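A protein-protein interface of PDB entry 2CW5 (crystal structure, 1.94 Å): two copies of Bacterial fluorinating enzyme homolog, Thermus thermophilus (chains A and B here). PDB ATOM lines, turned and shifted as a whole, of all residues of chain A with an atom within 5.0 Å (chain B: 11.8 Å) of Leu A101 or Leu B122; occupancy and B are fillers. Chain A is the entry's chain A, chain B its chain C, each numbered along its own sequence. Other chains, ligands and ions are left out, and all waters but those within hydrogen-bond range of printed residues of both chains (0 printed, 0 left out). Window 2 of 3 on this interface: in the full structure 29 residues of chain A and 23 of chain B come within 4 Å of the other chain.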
ATOM      1  N   PHE A  53       9.383  -2.811  -0.642  1.00  0.00           N
ATOM      2  CA  PHE A  53       9.292  -3.108  -2.071  1.00  0.00           C
ATOM      3  C   PHE A  53      10.380  -4.113  -2.466  1.00  0.00           C
ATOM      4  O   PHE A  53      10.125  -5.062  -3.209  1.00  0.00           O
ATOM      5  CB  PHE A  53       9.473  -1.815  -2.878  1.00  0.00           C
ATOM      6  CG  PHE A  53       9.394  -2.006  -4.371  1.00  0.00           C
ATOM      7  CD1 PHE A  53       8.168  -2.196  -5.003  1.00  0.00           C
ATOM      8  CD2 PHE A  53      10.549  -1.973  -5.147  1.00  0.00           C
ATOM      9  CE1 PHE A  53       8.093  -2.347  -6.386  1.00  0.00           C
ATOM     10  CE2 PHE A  53      10.489  -2.124  -6.529  1.00  0.00           C
ATOM     11  CZ  PHE A  53       9.250  -2.310  -7.152  1.00  0.00           C
ATOM     12  N   THR A  97       2.994   1.971   0.536  1.00  0.00           N
ATOM     13  CA  THR A  97       2.698   2.419  -0.824  1.00  0.00           C
ATOM     14  C   THR A  97       3.279   1.585  -1.955  1.00  0.00           C
ATOM     15  O   THR A  97       2.550   1.159  -2.848  1.00  0.00           O
ATOM     16  CB  THR A  97       3.137   3.892  -1.040  1.00  0.00           C
ATOM     17  OG1 THR A  97       2.393   4.745  -0.166  1.00  0.00           O
ATOM     18  CG2 THR A  97       2.878   4.327  -2.480  1.00  0.00           C
ATOM     19  N   LEU A  98       4.589   1.361  -1.930  1.00  0.00           N
ATOM     20  CA  LEU A  98       5.221   0.597  -2.995  1.00  0.00           C
ATOM     21  C   LEU A  98       4.870  -0.892  -2.933  1.00  0.00           C
ATOM     22  O   LEU A  98       4.743  -1.543  -3.965  1.00  0.00           O
ATOM     23  CB  LEU A  98       6.733   0.813  -2.952  1.00  0.00           C
ATOM     24  CG  LEU A  98       7.119   2.295  -3.058  1.00  0.00           C
ATOM     25  CD1 LEU A  98       8.617   2.480  -2.828  1.00  0.00           C
ATOM     26  CD2 LEU A  98       6.716   2.820  -4.438  1.00  0.00           C
ATOM     27  N   ALA A  99       4.701  -1.430  -1.728  1.00  0.00           N
ATOM     28  CA  ALA A  99       4.338  -2.837  -1.595  1.00  0.00           C
ATOM     29  C   ALA A  99       2.950  -3.040  -2.210  1.00  0.00           C
ATOM     30  O   ALA A  99       2.682  -4.048  -2.862  1.00  0.00           O
ATOM     31  CB  ALA A  99       4.323  -3.241  -0.120  1.00  0.00           C
ATOM     32  N   TRP A 100       2.070  -2.067  -2.006  1.00  0.00           N
ATOM     33  CA  TRP A 100       0.721  -2.163  -2.540  1.00  0.00           C
ATOM     34  C   TRP A 100       0.636  -1.997  -4.056  1.00  0.00           C
ATOM     35  O   TRP A 100      -0.393  -2.306  -4.656  1.00  0.00           O
ATOM     36  CB  TRP A 100      -0.197  -1.171  -1.835  1.00  0.00           C
ATOM     37  CG  TRP A 100      -0.446  -1.547  -0.405  1.00  0.00           C
ATOM     38  CD1 TRP A 100      -0.358  -2.798   0.148  1.00  0.00           C
ATOM     39  CD2 TRP A 100      -0.856  -0.672   0.649  1.00  0.00           C
ATOM     40  NE1 TRP A 100      -0.689  -2.752   1.485  1.00  0.00           N
ATOM     41  CE2 TRP A 100      -1.002  -1.459   1.816  1.00  0.00           C
ATOM     42  CE3 TRP A 100      -1.116   0.702   0.721  1.00  0.00           C
ATOM     43  CZ2 TRP A 100      -1.398  -0.915   3.040  1.00  0.00           C
ATOM     44  CZ3 TRP A 100      -1.509   1.243   1.943  1.00  0.00           C
ATOM     45  CH2 TRP A 100      -1.645   0.434   3.081  1.00  0.00           C
ATOM     46  N   LEU A 101       1.711  -1.513  -4.670  1.00  0.00           N
ATOM     47  CA  LEU A 101       1.749  -1.385  -6.129  1.00  0.00           C
ATOM     48  C   LEU A 101       1.940  -2.803  -6.651  1.00  0.00           C
ATOM     49  O   LEU A 101       1.404  -3.189  -7.692  1.00  0.00           O
ATOM     50  CB  LEU A 101       2.930  -0.517  -6.580  1.00  0.00           C
ATOM     51  CG  LEU A 101       2.830   0.999  -6.374  1.00  0.00           C
ATOM     52  CD1 LEU A 101       4.124   1.657  -6.817  1.00  0.00           C
ATOM     53  CD2 LEU A 101       1.651   1.561  -7.176  1.00  0.00           C
ATOM     54  N   LEU A 102       2.724  -3.585  -5.915  1.00  0.00           N
ATOM     55  CA  LEU A 102       2.972  -4.966  -6.295  1.00  0.00           C
ATOM     56  C   LEU A 102       1.798  -5.848  -5.877  1.00  0.00           C
ATOM     57  O   LEU A 102       1.452  -6.816  -6.569  1.00  0.00           O
ATOM     58  CB  LEU A 102       4.248  -5.485  -5.618  1.00  0.00           C
ATOM     59  CG  LEU A 102       5.580  -4.802  -5.936  1.00  0.00           C
ATOM     60  CD1 LEU A 102       6.693  -5.422  -5.114  1.00  0.00           C
ATOM     61  CD2 LEU A 102       5.881  -4.948  -7.420  1.00  0.00           C
ATOM     62  N   ASP A 103       1.185  -5.504  -4.747  1.00  0.00           N
ATOM     63  CA  ASP A 103       0.089  -6.291  -4.188  1.00  0.00           C
ATOM     64  C   ASP A 103      -1.069  -5.420  -3.683  1.00  0.00           C
ATOM     65  O   ASP A 103      -1.163  -5.122  -2.494  1.00  0.00           O
ATOM     66  CB  ASP A 103       0.671  -7.163  -3.061  1.00  0.00           C
ATOM     67  CG  ASP A 103      -0.371  -8.003  -2.348  1.00  0.00           C
ATOM     68  OD1 ASP A 103      -1.300  -8.513  -3.008  1.00  0.00           O
ATOM     69  OD2 ASP A 103      -0.244  -8.168  -1.113  1.00  0.00           O
ATOM     70  N   PRO A 104      -1.963  -4.993  -4.594  1.00  0.00           N
ATOM     71  CA  PRO A 104      -3.114  -4.155  -4.237  1.00  0.00           C
ATOM     72  C   PRO A 104      -3.992  -4.827  -3.184  1.00  0.00           C
ATOM     73  O   PRO A 104      -4.531  -5.906  -3.417  1.00  0.00           O
ATOM     74  CB  PRO A 104      -3.843  -3.981  -5.573  1.00  0.00           C
ATOM     75  CG  PRO A 104      -2.735  -4.032  -6.558  1.00  0.00           C
ATOM     76  CD  PRO A 104      -1.900  -5.188  -6.052  1.00  0.00           C
ATOM     77  N   LEU A 170       6.061   4.631  -9.552  1.00  0.00           N
ATOM     78  CA  LEU A 170       7.158   4.029 -10.293  1.00  0.00           C
ATOM     79  C   LEU A 170       6.709   4.234 -11.728  1.00  0.00           C
ATOM     80  O   LEU A 170       5.554   3.984 -12.057  1.00  0.00           O
ATOM     81  CB  LEU A 170       7.298   2.546  -9.949  1.00  0.00           C
ATOM     82  CG  LEU A 170       7.533   2.307  -8.454  1.00  0.00           C
ATOM     83  CD1 LEU A 170       7.764   0.830  -8.195  1.00  0.00           C
ATOM     84  CD2 LEU A 170       8.732   3.127  -7.988  1.00  0.00           C
ATOM     85  N   LEU A 192      11.601   2.630 -13.819  1.00  0.00           N
ATOM     86  CA  LEU A 192      11.582   1.179 -13.973  1.00  0.00           C
ATOM     87  C   LEU A 192      12.504   0.697 -15.093  1.00  0.00           C
ATOM     88  O   LEU A 192      12.727  -0.506 -15.243  1.00  0.00           O
ATOM     89  CB  LEU A 192      10.153   0.711 -14.270  1.00  0.00           C
ATOM     90  CG  LEU A 192       9.100   0.948 -13.176  1.00  0.00           C
ATOM     91  CD1 LEU A 192       7.694   0.869 -13.765  1.00  0.00           C
ATOM     92  CD2 LEU A 192       9.288  -0.072 -12.068  1.00  0.00           C
ATOM     93  N   ARG B 117      12.618 -17.157  -8.111  1.00  0.00           N
ATOM     94  CA  ARG B 117      11.601 -16.415  -8.850  1.00  0.00           C
ATOM     95  C   ARG B 117      10.790 -15.440  -7.996  1.00  0.00           C
ATOM     96  O   ARG B 117      10.166 -15.835  -7.013  1.00  0.00           O
ATOM     97  CB  ARG B 117      10.641 -17.394  -9.532  1.00  0.00           C
ATOM     98  CG  ARG B 117      11.296 -18.326 -10.538  1.00  0.00           C
ATOM     99  CD  ARG B 117      11.929 -17.537 -11.669  1.00  0.00           C
ATOM    100  NE  ARG B 117      10.990 -16.580 -12.252  1.00  0.00           N
ATOM    101  CZ  ARG B 117      11.288 -15.748 -13.244  1.00  0.00           C
ATOM    102  NH1 ARG B 117      10.371 -14.911 -13.711  1.00  0.00           N
ATOM    103  NH2 ARG B 117      12.504 -15.756 -13.774  1.00  0.00           N
ATOM    104  N   PRO B 118      10.791 -14.149  -8.362  1.00  0.00           N
ATOM    105  CA  PRO B 118      10.025 -13.164  -7.591  1.00  0.00           C
ATOM    106  C   PRO B 118       8.531 -13.478  -7.708  1.00  0.00           C
ATOM    107  O   PRO B 118       8.037 -13.764  -8.800  1.00  0.00           O
ATOM    108  CB  PRO B 118      10.409 -11.835  -8.248  1.00  0.00           C
ATOM    109  CG  PRO B 118      10.706 -12.235  -9.667  1.00  0.00           C
ATOM    110  CD  PRO B 118      11.502 -13.506  -9.480  1.00  0.00           C
ATOM    111  N   LYS B 119       7.822 -13.430  -6.583  1.00  0.00           N
ATOM    112  CA  LYS B 119       6.395 -13.745  -6.548  1.00  0.00           C
ATOM    113  C   LYS B 119       5.499 -12.651  -7.116  1.00  0.00           C
ATOM    114  O   LYS B 119       4.435 -12.931  -7.672  1.00  0.00           O
ATOM    115  CB  LYS B 119       5.985 -14.071  -5.112  1.00  0.00           C
ATOM    116  CG  LYS B 119       6.674 -15.318  -4.577  1.00  0.00           C
ATOM    117  CD  LYS B 119       6.804 -15.296  -3.063  1.00  0.00           C
ATOM    118  CE  LYS B 119       7.526 -16.537  -2.563  1.00  0.00           C
ATOM    119  NZ  LYS B 119       8.878 -16.693  -3.172  1.00  0.00           N
ATOM    120  N   ALA B 120       5.926 -11.405  -6.965  1.00  0.00           N
ATOM    121  CA  ALA B 120       5.165 -10.285  -7.486  1.00  0.00           C
ATOM    122  C   ALA B 120       6.043  -9.611  -8.529  1.00  0.00           C
ATOM    123  O   ALA B 120       7.272  -9.665  -8.438  1.00  0.00           O
ATOM    124  CB  ALA B 120       4.821  -9.312  -6.365  1.00  0.00           C
ATOM    125  N   ALA B 121       5.423  -8.986  -9.522  1.00  0.00           N
ATOM    126  CA  ALA B 121       6.193  -8.315 -10.561  1.00  0.00           C
ATOM    127  C   ALA B 121       5.331  -7.398 -11.412  1.00  0.00           C
ATOM    128  O   ALA B 121       4.290  -7.806 -11.926  1.00  0.00           O
ATOM    129  CB  ALA B 121       6.882  -9.349 -11.446  1.00  0.00           C
ATOM    130  N   LEU B 122       5.768  -6.152 -11.551  1.00  0.00           N
ATOM    131  CA  LEU B 122       5.046  -5.182 -12.359  1.00  0.00           C
ATOM    132  C   LEU B 122       5.204  -5.586 -13.825  1.00  0.00           C
ATOM    133  O   LEU B 122       6.105  -6.352 -14.170  1.00  0.00           O
ATOM    134  CB  LEU B 122       5.616  -3.783 -12.123  1.00  0.00           C
ATOM    135  CG  LEU B 122       5.408  -3.225 -10.713  1.00  0.00           C
ATOM    136  CD1 LEU B 122       6.241  -1.965 -10.526  1.00  0.00           C
ATOM    137  CD2 LEU B 122       3.928  -2.939 -10.495  1.00  0.00           C
ATOM    138  N   PRO B 123       4.325  -5.084 -14.706  1.00  0.00           N
ATOM    139  CA  PRO B 123       4.395  -5.417 -16.135  1.00  0.00           C
ATOM    140  C   PRO B 123       5.793  -5.272 -16.739  1.00  0.00           C
ATOM    141  O   PRO B 123       6.370  -4.186 -16.740  1.00  0.00           O
ATOM    142  CB  PRO B 123       3.390  -4.451 -16.756  1.00  0.00           C
ATOM    143  CG  PRO B 123       2.349  -4.336 -15.679  1.00  0.00           C
ATOM    144  CD  PRO B 123       3.201  -4.169 -14.437  1.00  0.00           C
ATOM    145  N   GLY B 124       6.328  -6.380 -17.247  1.00  0.00           N
ATOM    146  CA  GLY B 124       7.646  -6.370 -17.860  1.00  0.00           C
ATOM    147  C   GLY B 124       8.776  -6.069 -16.898  1.00  0.00           C
ATOM    148  O   GLY B 124       9.882  -5.735 -17.321  1.00  0.00           O
ATOM    149  N   TRP B 125       8.497  -6.193 -15.603  1.00  0.00           N
ATOM    150  CA  TRP B 125       9.481  -5.924 -14.555  1.00  0.00           C
ATOM    151  C   TRP B 125      10.423  -7.097 -14.319  1.00  0.00           C
ATOM    152  O   TRP B 125      10.025  -8.259 -14.398  1.00  0.00           O
ATOM    153  CB  TRP B 125       8.764  -5.592 -13.242  1.00  0.00           C
ATOM    154  CG  TRP B 125       9.674  -5.422 -12.057  1.00  0.00           C
ATOM    155  CD1 TRP B 125      10.186  -4.250 -11.572  1.00  0.00           C
ATOM    156  CD2 TRP B 125      10.170  -6.460 -11.201  1.00  0.00           C
ATOM    157  NE1 TRP B 125      10.965  -4.493 -10.464  1.00  0.00           N
ATOM    158  CE2 TRP B 125      10.973  -5.842 -10.215  1.00  0.00           C
ATOM    159  CE3 TRP B 125      10.013  -7.854 -11.170  1.00  0.00           C
ATOM    160  CZ2 TRP B 125      11.618  -6.571  -9.207  1.00  0.00           C
ATOM    161  CZ3 TRP B 125      10.655  -8.579 -10.168  1.00  0.00           C
ATOM    162  CH2 TRP B 125      11.447  -7.934  -9.200  1.00  0.00           C
ATOM    163  N   ALA B 126      11.676  -6.775 -14.015  1.00  0.00           N
ATOM    164  CA  ALA B 126      12.699  -7.775 -13.741  1.00  0.00           C
ATOM    165  C   ALA B 126      13.864  -7.115 -13.003  1.00  0.00           C
ATOM    166  O   ALA B 126      14.302  -6.022 -13.362  1.00  0.00           O
ATOM    167  CB  ALA B 126      13.188  -8.399 -15.040  1.00  0.00           C
ATOM    168  N   PRO B 127      14.378  -7.774 -11.953  1.00  0.00           N
ATOM    169  CA  PRO B 127      15.495  -7.207 -11.193  1.00  0.00           C
ATOM    170  C   PRO B 127      16.778  -7.171 -12.019  1.00  0.00           C
ATOM    171  O   PRO B 127      16.925  -7.924 -12.984  1.00  0.00           O
ATOM    172  CB  PRO B 127      15.596  -8.140  -9.988  1.00  0.00           C
ATOM    173  CG  PRO B 127      15.179  -9.458 -10.564  1.00  0.00           C
ATOM    174  CD  PRO B 127      13.983  -9.087 -11.410  1.00  0.00           C
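Leu A101 touches just one residue of chain B: Leu B122. Of chain A, only Leu A101 (3.8 Å), Leu A102 (3.7 Å), Leu A170 (3.9 Å) and Leu A192 (3.9 Å) come within 4 Å of Leu B122. No residue of chain B comes within 4 Å of Leu A98. Ala A99 touches none of the printed residues of chain B. Leu A102 touches two residues of chain B. No residue of chain B comes within 4 Å of Pro A104. Leu A170 touches just one residue of chain B: Leu B122 (3.9 Å). Printed residues of chain A within 4 Å of Ala B120: Leu A102 (3.9 Å). Printed residues of chain B within 4 Å of Leu A192: Leu B122 (3.9 Å). The nearest residue of chain B that does not touch Leu A101 is Ala B121 (6.9 Å). The nearest printed residue of chain B that does not touch Leu A192 is Trp B125 (4.3 Å).
No position is printed for both chains. Of the 5 pairs that touch across the chains among the printed residues, none has its exchanged pair printed and touching as well.
Printed residues of chain A that touch a printed residue of chain B: Leu A101, Leu A102, Leu A170 and Leu A192. Printed residues of chain B that touch a printed residue of chain A: Ala B120 and Leu B122. Hydrophobic or aromatic side chains of chain B within 4 Å of the printed part of chain A: Ala B120 and Leu B122. Among the printed residues, 5 pairs touch across the chains. Among the printed residues, no Asp or Glu carboxylate lies within 4 Å of a Lys or Arg side-chain nitrogen of the other chain.
Among the printed residues, merely in contact across the chains: Leu A102 with Leu B122, Leu A101 with Leu B122, Leu A192 with Leu B122, Leu A102 with Ala B120 and Leu A170 with Leu B122.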
